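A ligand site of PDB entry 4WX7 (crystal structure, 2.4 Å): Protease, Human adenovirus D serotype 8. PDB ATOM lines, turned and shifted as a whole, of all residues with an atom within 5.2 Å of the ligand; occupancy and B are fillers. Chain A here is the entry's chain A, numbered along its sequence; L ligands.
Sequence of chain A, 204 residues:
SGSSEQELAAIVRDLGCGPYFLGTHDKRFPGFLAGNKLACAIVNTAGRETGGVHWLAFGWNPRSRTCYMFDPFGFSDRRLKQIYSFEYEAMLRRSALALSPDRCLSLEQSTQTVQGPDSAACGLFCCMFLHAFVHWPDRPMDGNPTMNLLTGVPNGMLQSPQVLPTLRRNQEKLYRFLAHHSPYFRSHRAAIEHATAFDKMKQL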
ATOM      1  N   SER A   1     -21.350 -20.201  -0.655  1.00  0.00           N
ATOM      2  CA  SER A   1     -21.667 -19.175   0.408  1.00  0.00           C
ATOM      3  C   SER A   1     -22.832 -19.531   1.356  1.00  0.00           C
ATOM      4  O   SER A   1     -23.994 -19.313   1.018  1.00  0.00           O
ATOM      5  CB  SER A   1     -21.921 -17.798  -0.235  1.00  0.00           C
ATOM      6  OG  SER A   1     -22.131 -16.810   0.772  1.00  0.00           O
ATOM      7  N   GLY A   2     -22.522 -20.037   2.540  1.00  0.00           N
ATOM      8  CA  GLY A   2     -23.550 -20.438   3.506  1.00  0.00           C
ATOM      9  C   GLY A   2     -23.844 -21.929   3.487  1.00  0.00           C
ATOM     10  O   GLY A   2     -23.058 -22.726   2.971  1.00  0.00           O
ATOM     11  N   SER A   3     -24.984 -22.320   4.058  1.00  0.00           N
ATOM     12  CA  SER A   3     -25.473 -23.691   3.947  1.00  0.00           C
ATOM     13  C   SER A   3     -26.988 -23.784   3.677  1.00  0.00           C
ATOM     14  O   SER A   3     -27.770 -23.058   4.268  1.00  0.00           O
ATOM     15  CB  SER A   3     -24.997 -24.587   5.124  1.00  0.00           C
ATOM     16  OG  SER A   3     -24.599 -23.890   6.321  1.00  0.00           O
ATOM     17  N   SER A   4     -27.382 -24.664   2.767  1.00  0.00           N
ATOM     18  CA  SER A   4     -28.776 -24.832   2.273  1.00  0.00           C
ATOM     19  C   SER A   4     -29.687 -25.742   3.118  1.00  0.00           C
ATOM     20  O   SER A   4     -29.221 -26.709   3.671  1.00  0.00           O
ATOM     21  CB  SER A   4     -28.760 -25.378   0.830  1.00  0.00           C
ATOM     22  OG  SER A   4     -28.615 -26.813   0.792  1.00  0.00           O
ATOM     23  N   GLU A   5     -31.003 -25.486   3.117  1.00  0.00           N
ATOM     24  CA  GLU A   5     -31.964 -26.300   3.905  1.00  0.00           C
ATOM     25  C   GLU A   5     -31.904 -27.807   3.678  1.00  0.00           C
ATOM     26  O   GLU A   5     -32.206 -28.601   4.599  1.00  0.00           O
ATOM     27  CB  GLU A   5     -33.415 -25.841   3.710  1.00  0.00           C
ATOM     28  CG  GLU A   5     -34.229 -26.655   2.729  1.00  0.00           C
ATOM     29  CD  GLU A   5     -35.564 -25.988   2.473  1.00  0.00           C
ATOM     30  OE1 GLU A   5     -35.535 -24.907   1.809  1.00  0.00           O
ATOM     31  OE2 GLU A   5     -36.638 -26.512   2.912  1.00  0.00           O
ATOM     32  N   GLN A   6     -31.558 -28.189   2.450  1.00  0.00           N
ATOM     33  CA  GLN A   6     -31.411 -29.580   2.079  1.00  0.00           C
ATOM     34  C   GLN A   6     -30.189 -30.166   2.833  1.00  0.00           C
ATOM     35  O   GLN A   6     -30.195 -31.276   3.330  1.00  0.00           O
ATOM     36  CB  GLN A   6     -31.230 -29.689   0.548  1.00  0.00           C
ATOM     37  CG  GLN A   6     -32.490 -29.396  -0.285  1.00  0.00           C
ATOM     38  CD  GLN A   6     -32.689 -27.926  -0.704  1.00  0.00           C
ATOM     39  OE1 GLN A   6     -33.840 -27.493  -0.885  1.00  0.00           O
ATOM     40  NE2 GLN A   6     -31.576 -27.142  -0.830  1.00  0.00           N
ATOM     41  N   THR A  24     -36.256 -27.496   8.488  1.00  0.00           N
ATOM     42  CA  THR A  24     -35.686 -26.163   8.567  1.00  0.00           C
ATOM     43  C   THR A  24     -36.736 -25.179   8.094  1.00  0.00           C
ATOM     44  O   THR A  24     -37.577 -25.519   7.253  1.00  0.00           O
ATOM     45  CB  THR A  24     -34.347 -26.043   7.810  1.00  0.00           C
ATOM     46  OG1 THR A  24     -34.570 -25.960   6.401  1.00  0.00           O
ATOM     47  CG2 THR A  24     -33.458 -27.261   8.136  1.00  0.00           C
ATOM     48  N   HIS A  25     -36.731 -23.982   8.673  1.00  0.00           N
ATOM     49  CA  HIS A  25     -37.728 -22.968   8.314  1.00  0.00           C
ATOM     50  C   HIS A  25     -37.132 -21.588   8.152  1.00  0.00           C
ATOM     51  O   HIS A  25     -36.076 -21.280   8.713  1.00  0.00           O
ATOM     52  CB  HIS A  25     -38.781 -22.834   9.400  1.00  0.00           C
ATOM     53  CG  HIS A  25     -39.745 -23.955   9.437  1.00  0.00           C
ATOM     54  ND1 HIS A  25     -39.420 -25.180   9.959  1.00  0.00           N
ATOM     55  CD2 HIS A  25     -41.038 -24.024   9.040  1.00  0.00           C
ATOM     56  CE1 HIS A  25     -40.476 -25.973   9.874  1.00  0.00           C
ATOM     57  NE2 HIS A  25     -41.465 -25.295   9.321  1.00  0.00           N
ATOM     58  N   ASP A  26     -37.847 -20.758   7.414  1.00  0.00           N
ATOM     59  CA  ASP A  26     -37.665 -19.334   7.458  1.00  0.00           C
ATOM     60  C   ASP A  26     -38.205 -18.785   8.798  1.00  0.00           C
ATOM     61  O   ASP A  26     -38.719 -19.585   9.601  1.00  0.00           O
ATOM     62  CB  ASP A  26     -38.319 -18.682   6.228  1.00  0.00           C
ATOM     63  CG  ASP A  26     -39.826 -18.541   6.342  1.00  0.00           C
ATOM     64  OD1 ASP A  26     -40.418 -18.768   7.416  1.00  0.00           O
ATOM     65  OD2 ASP A  26     -40.439 -18.151   5.323  1.00  0.00           O
ATOM     66  N   ASN A  44     -34.498 -19.900  10.112  1.00  0.00           N
ATOM     67  CA  ASN A  44     -33.804 -18.776   9.584  1.00  0.00           C
ATOM     68  C   ASN A  44     -34.347 -17.495  10.235  1.00  0.00           C
ATOM     69  O   ASN A  44     -35.494 -17.454  10.711  1.00  0.00           O
ATOM     70  CB  ASN A  44     -34.027 -18.692   8.103  1.00  0.00           C
ATOM     71  CG  ASN A  44     -32.896 -17.982   7.413  1.00  0.00           C
ATOM     72  OD1 ASN A  44     -32.895 -16.750   7.268  1.00  0.00           O
ATOM     73  ND2 ASN A  44     -31.947 -18.744   6.967  1.00  0.00           N
ATOM     74  N   ALA A  46     -34.505 -14.539   8.495  1.00  0.00           N
ATOM     75  CA  ALA A  46     -35.288 -13.852   7.446  1.00  0.00           C
ATOM     76  C   ALA A  46     -36.419 -14.729   6.873  1.00  0.00           C
ATOM     77  O   ALA A  46     -36.641 -15.839   7.356  1.00  0.00           O
ATOM     78  CB  ALA A  46     -34.365 -13.397   6.315  1.00  0.00           C
ATOM     79  N   GLY A  47     -37.152 -14.201   5.879  1.00  0.00           N
ATOM     80  CA  GLY A  47     -38.161 -14.977   5.147  1.00  0.00           C
ATOM     81  C   GLY A  47     -37.514 -15.776   4.027  1.00  0.00           C
ATOM     82  O   GLY A  47     -36.341 -15.509   3.642  1.00  0.00           O
ATOM     83  N   ARG A  48     -38.250 -16.753   3.472  1.00  0.00           N
ATOM     84  CA  ARG A  48     -37.704 -17.554   2.336  1.00  0.00           C
ATOM     85  C   ARG A  48     -37.410 -16.619   1.172  1.00  0.00           C
ATOM     86  O   ARG A  48     -36.442 -16.789   0.453  1.00  0.00           O
ATOM     87  CB  ARG A  48     -38.684 -18.656   1.916  1.00  0.00           C
ATOM     88  CG  ARG A  48     -38.296 -19.417   0.648  1.00  0.00           C
ATOM     89  CD  ARG A  48     -39.158 -20.654   0.392  1.00  0.00           C
ATOM     90  NE  ARG A  48     -38.767 -21.800   1.222  1.00  0.00           N
ATOM     91  CZ  ARG A  48     -38.054 -22.828   0.771  1.00  0.00           C
ATOM     92  NH1 ARG A  48     -37.723 -23.815   1.591  1.00  0.00           N
ATOM     93  NH2 ARG A  48     -37.676 -22.878  -0.509  1.00  0.00           N
ATOM     94  N   THR A  50     -36.159 -13.740   0.989  1.00  0.00           N
ATOM     95  CA  THR A  50     -34.853 -13.023   1.021  1.00  0.00           C
ATOM     96  C   THR A  50     -33.716 -13.912   0.501  1.00  0.00           C
ATOM     97  O   THR A  50     -32.560 -13.442   0.303  1.00  0.00           O
ATOM     98  CB  THR A  50     -34.458 -12.564   2.447  1.00  0.00           C
ATOM     99  OG1 THR A  50     -34.211 -13.705   3.289  1.00  0.00           O
ATOM    100  CG2 THR A  50     -35.571 -11.593   3.078  1.00  0.00           C
ATOM    101  N   GLY A  51     -34.038 -15.189   0.290  1.00  0.00           N
ATOM    102  CA  GLY A  51     -33.046 -16.183  -0.091  1.00  0.00           C
ATOM    103  C   GLY A  51     -32.119 -16.666   1.030  1.00  0.00           C
ATOM    104  O   GLY A  51     -31.322 -17.572   0.812  1.00  0.00           O
ATOM    105  N   GLY A  52     -32.232 -16.077   2.233  1.00  0.00           N
ATOM    106  CA  GLY A  52     -31.606 -16.646   3.444  1.00  0.00           C
ATOM    107  C   GLY A  52     -30.501 -15.800   4.059  1.00  0.00           C
ATOM    108  O   GLY A  52     -29.672 -15.288   3.362  1.00  0.00           O
ATOM    109  N   VAL A  53     -30.531 -15.626   5.378  1.00  0.00           N
ATOM    110  CA  VAL A  53     -29.515 -14.827   6.076  1.00  0.00           C
ATOM    111  C   VAL A  53     -28.755 -15.568   7.191  1.00  0.00           C
ATOM    112  O   VAL A  53     -27.553 -15.742   7.068  1.00  0.00           O
ATOM    113  CB  VAL A  53     -30.089 -13.491   6.567  1.00  0.00           C
ATOM    114  CG1 VAL A  53     -28.987 -12.641   7.190  1.00  0.00           C
ATOM    115  CG2 VAL A  53     -30.716 -12.743   5.406  1.00  0.00           C
ATOM    116  N   HIS A  54     -29.459 -15.995   8.239  1.00  0.00           N
ATOM    117  CA  HIS A  54     -28.838 -16.589   9.462  1.00  0.00           C
ATOM    118  C   HIS A  54     -29.608 -17.793  10.001  1.00  0.00           C
ATOM    119  O   HIS A  54     -30.835 -17.765  10.153  1.00  0.00           O
ATOM    120  CB  HIS A  54     -28.749 -15.545  10.583  1.00  0.00           C
ATOM    121  CG  HIS A  54     -27.830 -15.919  11.715  1.00  0.00           C
ATOM    122  ND1 HIS A  54     -26.532 -16.313  11.530  1.00  0.00           N
ATOM    123  CD2 HIS A  54     -28.037 -15.908  13.060  1.00  0.00           C
ATOM    124  CE1 HIS A  54     -25.982 -16.574  12.708  1.00  0.00           C
ATOM    125  NE2 HIS A  54     -26.873 -16.340  13.652  1.00  0.00           N
ATOM    126  N   TRP A  55     -28.871 -18.831  10.340  1.00  0.00           N
ATOM    127  CA  TRP A  55     -29.450 -20.020  10.937  1.00  0.00           C
ATOM    128  C   TRP A  55     -29.472 -19.952  12.468  1.00  0.00           C
ATOM    129  O   TRP A  55     -28.458 -19.558  13.064  1.00  0.00           O
ATOM    130  CB  TRP A  55     -28.699 -21.243  10.434  1.00  0.00           C
ATOM    131  CG  TRP A  55     -28.950 -21.609   8.911  1.00  0.00           C
ATOM    132  CD1 TRP A  55     -27.998 -21.841   7.967  1.00  0.00           C
ATOM    133  CD2 TRP A  55     -30.217 -21.827   8.255  1.00  0.00           C
ATOM    134  NE1 TRP A  55     -28.576 -22.179   6.752  1.00  0.00           N
ATOM    135  CE2 TRP A  55     -29.937 -22.175   6.910  1.00  0.00           C
ATOM    136  CE3 TRP A  55     -31.546 -21.749   8.674  1.00  0.00           C
ATOM    137  CZ2 TRP A  55     -30.932 -22.465   5.982  1.00  0.00           C
ATOM    138  CZ3 TRP A  55     -32.544 -22.034   7.755  1.00  0.00           C
ATOM    139  CH2 TRP A  55     -32.227 -22.381   6.413  1.00  0.00           C
ATOM    140  N   PHE A  73     -23.984 -17.176  17.671  1.00  0.00           N
ATOM    141  CA  PHE A  73     -23.359 -15.911  18.057  1.00  0.00           C
ATOM    142  C   PHE A  73     -23.721 -15.523  19.491  1.00  0.00           C
ATOM    143  O   PHE A  73     -23.076 -14.689  20.107  1.00  0.00           O
ATOM    144  CB  PHE A  73     -23.794 -14.774  17.094  1.00  0.00           C
ATOM    145  CG  PHE A  73     -23.108 -14.797  15.757  1.00  0.00           C
ATOM    146  CD1 PHE A  73     -23.820 -14.557  14.597  1.00  0.00           C
ATOM    147  CD2 PHE A  73     -21.734 -15.045  15.658  1.00  0.00           C
ATOM    148  CE1 PHE A  73     -23.184 -14.532  13.346  1.00  0.00           C
ATOM    149  CE2 PHE A  73     -21.115 -15.063  14.410  1.00  0.00           C
ATOM    150  CZ  PHE A  73     -21.833 -14.799  13.247  1.00  0.00           C
ATOM    151  N   GLN A 115     -19.089 -18.794  17.308  1.00  0.00           N
ATOM    152  CA  GLN A 115     -18.835 -18.507  15.913  1.00  0.00           C
ATOM    153  C   GLN A 115     -17.949 -17.240  15.650  1.00  0.00           C
ATOM    154  O   GLN A 115     -18.218 -16.162  16.181  1.00  0.00           O
ATOM    155  CB  GLN A 115     -20.172 -18.409  15.173  1.00  0.00           C
ATOM    156  CG  GLN A 115     -20.053 -18.762  13.719  1.00  0.00           C
ATOM    157  CD  GLN A 115     -21.335 -18.588  12.927  1.00  0.00           C
ATOM    158  OE1 GLN A 115     -21.289 -18.213  11.761  1.00  0.00           O
ATOM    159  NE2 GLN A 115     -22.471 -18.868  13.536  1.00  0.00           N
ATOM    160  N   SER A 119     -17.436 -15.989   9.898  1.00  0.00           N
ATOM    161  CA  SER A 119     -17.716 -17.386   9.575  1.00  0.00           C
ATOM    162  C   SER A 119     -19.105 -17.544   8.887  1.00  0.00           C
ATOM    163  O   SER A 119     -20.047 -16.792   9.186  1.00  0.00           O
ATOM    164  CB  SER A 119     -17.616 -18.255  10.850  1.00  0.00           C
ATOM    165  OG  SER A 119     -17.872 -19.616  10.566  1.00  0.00           O
ATOM    166  N   ALA A 120     -19.217 -18.493   7.958  1.00  0.00           N
ATOM    167  CA  ALA A 120     -20.508 -18.776   7.374  1.00  0.00           C
ATOM    168  C   ALA A 120     -20.996 -20.180   7.735  1.00  0.00           C
ATOM    169  O   ALA A 120     -21.757 -20.768   6.994  1.00  0.00           O
ATOM    170  CB  ALA A 120     -20.506 -18.558   5.877  1.00  0.00           C
ATOM    171  N   ALA A 121     -20.580 -20.673   8.907  1.00  0.00           N
ATOM    172  CA  ALA A 121     -20.944 -21.992   9.417  1.00  0.00           C
ATOM    173  C   ALA A 121     -22.153 -21.984  10.279  1.00  0.00           C
ATOM    174  O   ALA A 121     -22.449 -22.999  10.874  1.00  0.00           O
ATOM    175  CB  ALA A 121     -19.781 -22.583  10.222  1.00  0.00           C
ATOM    176  N   CYS A 122     -22.888 -20.881  10.384  1.00  0.00           N
ATOM    177  CA  CYS A 122     -23.960 -20.853  11.398  1.00  0.00           C
ATOM    178  C   CYS A 122     -24.822 -22.089  11.344  1.00  0.00           C
ATOM    179  O   CYS A 122     -25.120 -22.710  12.380  1.00  0.00           O
ATOM    180  CB  CYS A 122     -24.844 -19.610  11.300  1.00  0.00           C
ATOM    181  SG  CYS A 122     -25.662 -19.383   9.710  1.00  0.00           S
ATOM    182  N   GLY A 123     -25.212 -22.473  10.133  1.00  0.00           N
ATOM    183  CA  GLY A 123     -26.198 -23.517   9.954  1.00  0.00           C
ATOM    184  C   GLY A 123     -25.727 -24.783  10.616  1.00  0.00           C
ATOM    185  O   GLY A 123     -26.530 -25.539  11.197  1.00  0.00           O
HETATM  186  C1  LIG L   1     -30.104 -21.519   0.168  1.00  0.00           C
HETATM  187  C2  LIG L   1     -31.059 -21.462   1.214  1.00  0.00           C
HETATM  188  C3  LIG L   1     -30.735 -20.799   2.422  1.00  0.00           C
HETATM  189  C4  LIG L   1     -29.132 -19.499   3.920  1.00  0.00           C
HETATM  190  C5  LIG L   1     -34.376 -19.779   2.853  1.00  0.00           C
HETATM  191  C6  LIG L   1     -34.953 -19.620   4.105  1.00  0.00           C
HETATM  192  C7  LIG L   1     -35.464 -20.716   4.823  1.00  0.00           C
HETATM  193  C8  LIG L   1     -35.374 -21.986   4.248  1.00  0.00           C
HETATM  194  C9  LIG L   1     -34.793 -22.134   2.969  1.00  0.00           C
HETATM  195  C10 LIG L   1     -27.519 -18.714   5.628  1.00  0.00           C
HETATM  196  C11 LIG L   1     -26.216 -19.355   6.001  1.00  0.00           C
HETATM  197  C12 LIG L   1     -25.196 -17.649   7.571  1.00  0.00           C
HETATM  198  C13 LIG L   1     -29.487 -22.319  -2.170  1.00  0.00           C
HETATM  199  C14 LIG L   1     -33.453 -19.834   0.099  1.00  0.00           C
HETATM  200  C15 LIG L   1     -34.648 -21.991  -0.091  1.00  0.00           C
HETATM  201  C16 LIG L   1     -24.818 -18.062   8.949  1.00  0.00           C
HETATM  202  C17 LIG L   1     -29.478 -20.199   2.615  1.00  0.00           C
HETATM  203  C18 LIG L   1     -28.549 -20.287   1.574  1.00  0.00           C
HETATM  204  C19 LIG L   1     -28.833 -20.936   0.363  1.00  0.00           C
HETATM  205  C20 LIG L   1     -32.439 -22.053   1.002  1.00  0.00           C
HETATM  206  C21 LIG L   1     -33.686 -21.205   0.844  1.00  0.00           C
HETATM  207  O1  LIG L   1     -32.627 -23.241   0.919  1.00  0.00           O
HETATM  208  C22 LIG L   1     -34.307 -21.037   2.240  1.00  0.00           C
HETATM  209  O2  LIG L   1     -30.406 -22.193  -1.038  1.00  0.00           O
HETATM  210 CL1  LIG L   1     -35.002 -18.012   4.773  1.00  0.00          CL
HETATM  211 CL2  LIG L   1     -36.027 -23.388   5.079  1.00  0.00          CL
HETATM  212  N1  LIG L   1     -27.865 -19.397   4.362  1.00  0.00           N
HETATM  213  O3  LIG L   1     -30.047 -19.040   4.572  1.00  0.00           O
HETATM  214  O4  LIG L   1     -26.039 -20.428   5.491  1.00  0.00           O
HETATM  215  N2  LIG L   1     -25.227 -18.863   6.776  1.00  0.00           N
HETATM  216  N3  LIG L   1     -23.928 -17.493   9.525  1.00  0.00           N
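The side-chain sulfur of Cys 122 is bonded to a carbon (C16) of the ligand, at 1.7 Å.
An oxygen (O4) of the ligand sits at hydrogen-bond distance from the backbone NH (N) of Ser 3.
The side-chain amide nitrogen (ND2) of Asn 44 lies within hydrogen-bond range of an oxygen (O3) of the ligand, 3.1 Å away.
NE1 of Trp 55 lies within hydrogen-bond range of O4 of the ligand (3.3 Å).
N3 of the ligand sits at hydrogen-bond distance from ND1 of His 54, at 3.5 Å.
SG of Cys 122 sits at hydrogen-bond distance from ND1 of His 54 (3.7 Å).
N of Cys 122 sits at hydrogen-bond distance from OE1 of Gln 115 (3.4 Å).
The backbone carbonyl oxygen (O) of Ser 3 is in hydrogen-bond range of the indole nitrogen (NE1) of Trp 55, 2.8 Å away.
O of Gly 47 lies within hydrogen-bond range of OG1 of Thr 50.
The backbone carbonyl oxygen (O) of His 25 is in hydrogen-bond range of the backbone NH (N) of Asn 44 (2.5 Å).
The backbone NH of Gly 52 lies close to the side-chain hydroxyl of Thr 50.
The backbone NH (N) of Arg 48 is in hydrogen-bond range of the side-chain carboxylate (OD2) of Asp 26 (3.2 Å).
OG of Ser 119 lies within hydrogen-bond range of N of Ala 121, 3.3 Å away.
O1 of the ligand lies close to OE1 of Glu 5.
CA of Gly 2 touches O4 of the ligand, at 3.2 Å.
OG1 of Thr 24 touches CL2 of the ligand (3.2 Å).
His 25 touches the ligand.
Asp 26 touches the ligand.
Ala 46 touches the ligand (O to CL1, 3.8 Å).
Gly 47 touches the ligand.
NH2 of Arg 48 touches C15 of the ligand, 3.2 Å away.
O of Gly 51 touches C14 of the ligand (3.2 Å).
CA of Gly 52 touches O3 of the ligand, 3.1 Å away.
Val 53 touches the ligand (O to C12, 3.1 Å).
Gln 115 touches the ligand.
Ser 119 touches the ligand.
Ala 120 touches the ligand.
Hydrophobic or aromatic side chains that line the ligand: His 54 and Trp 55.
The nearest printed residue that does not touch the ligand is Ser 4 (4.04 Å).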
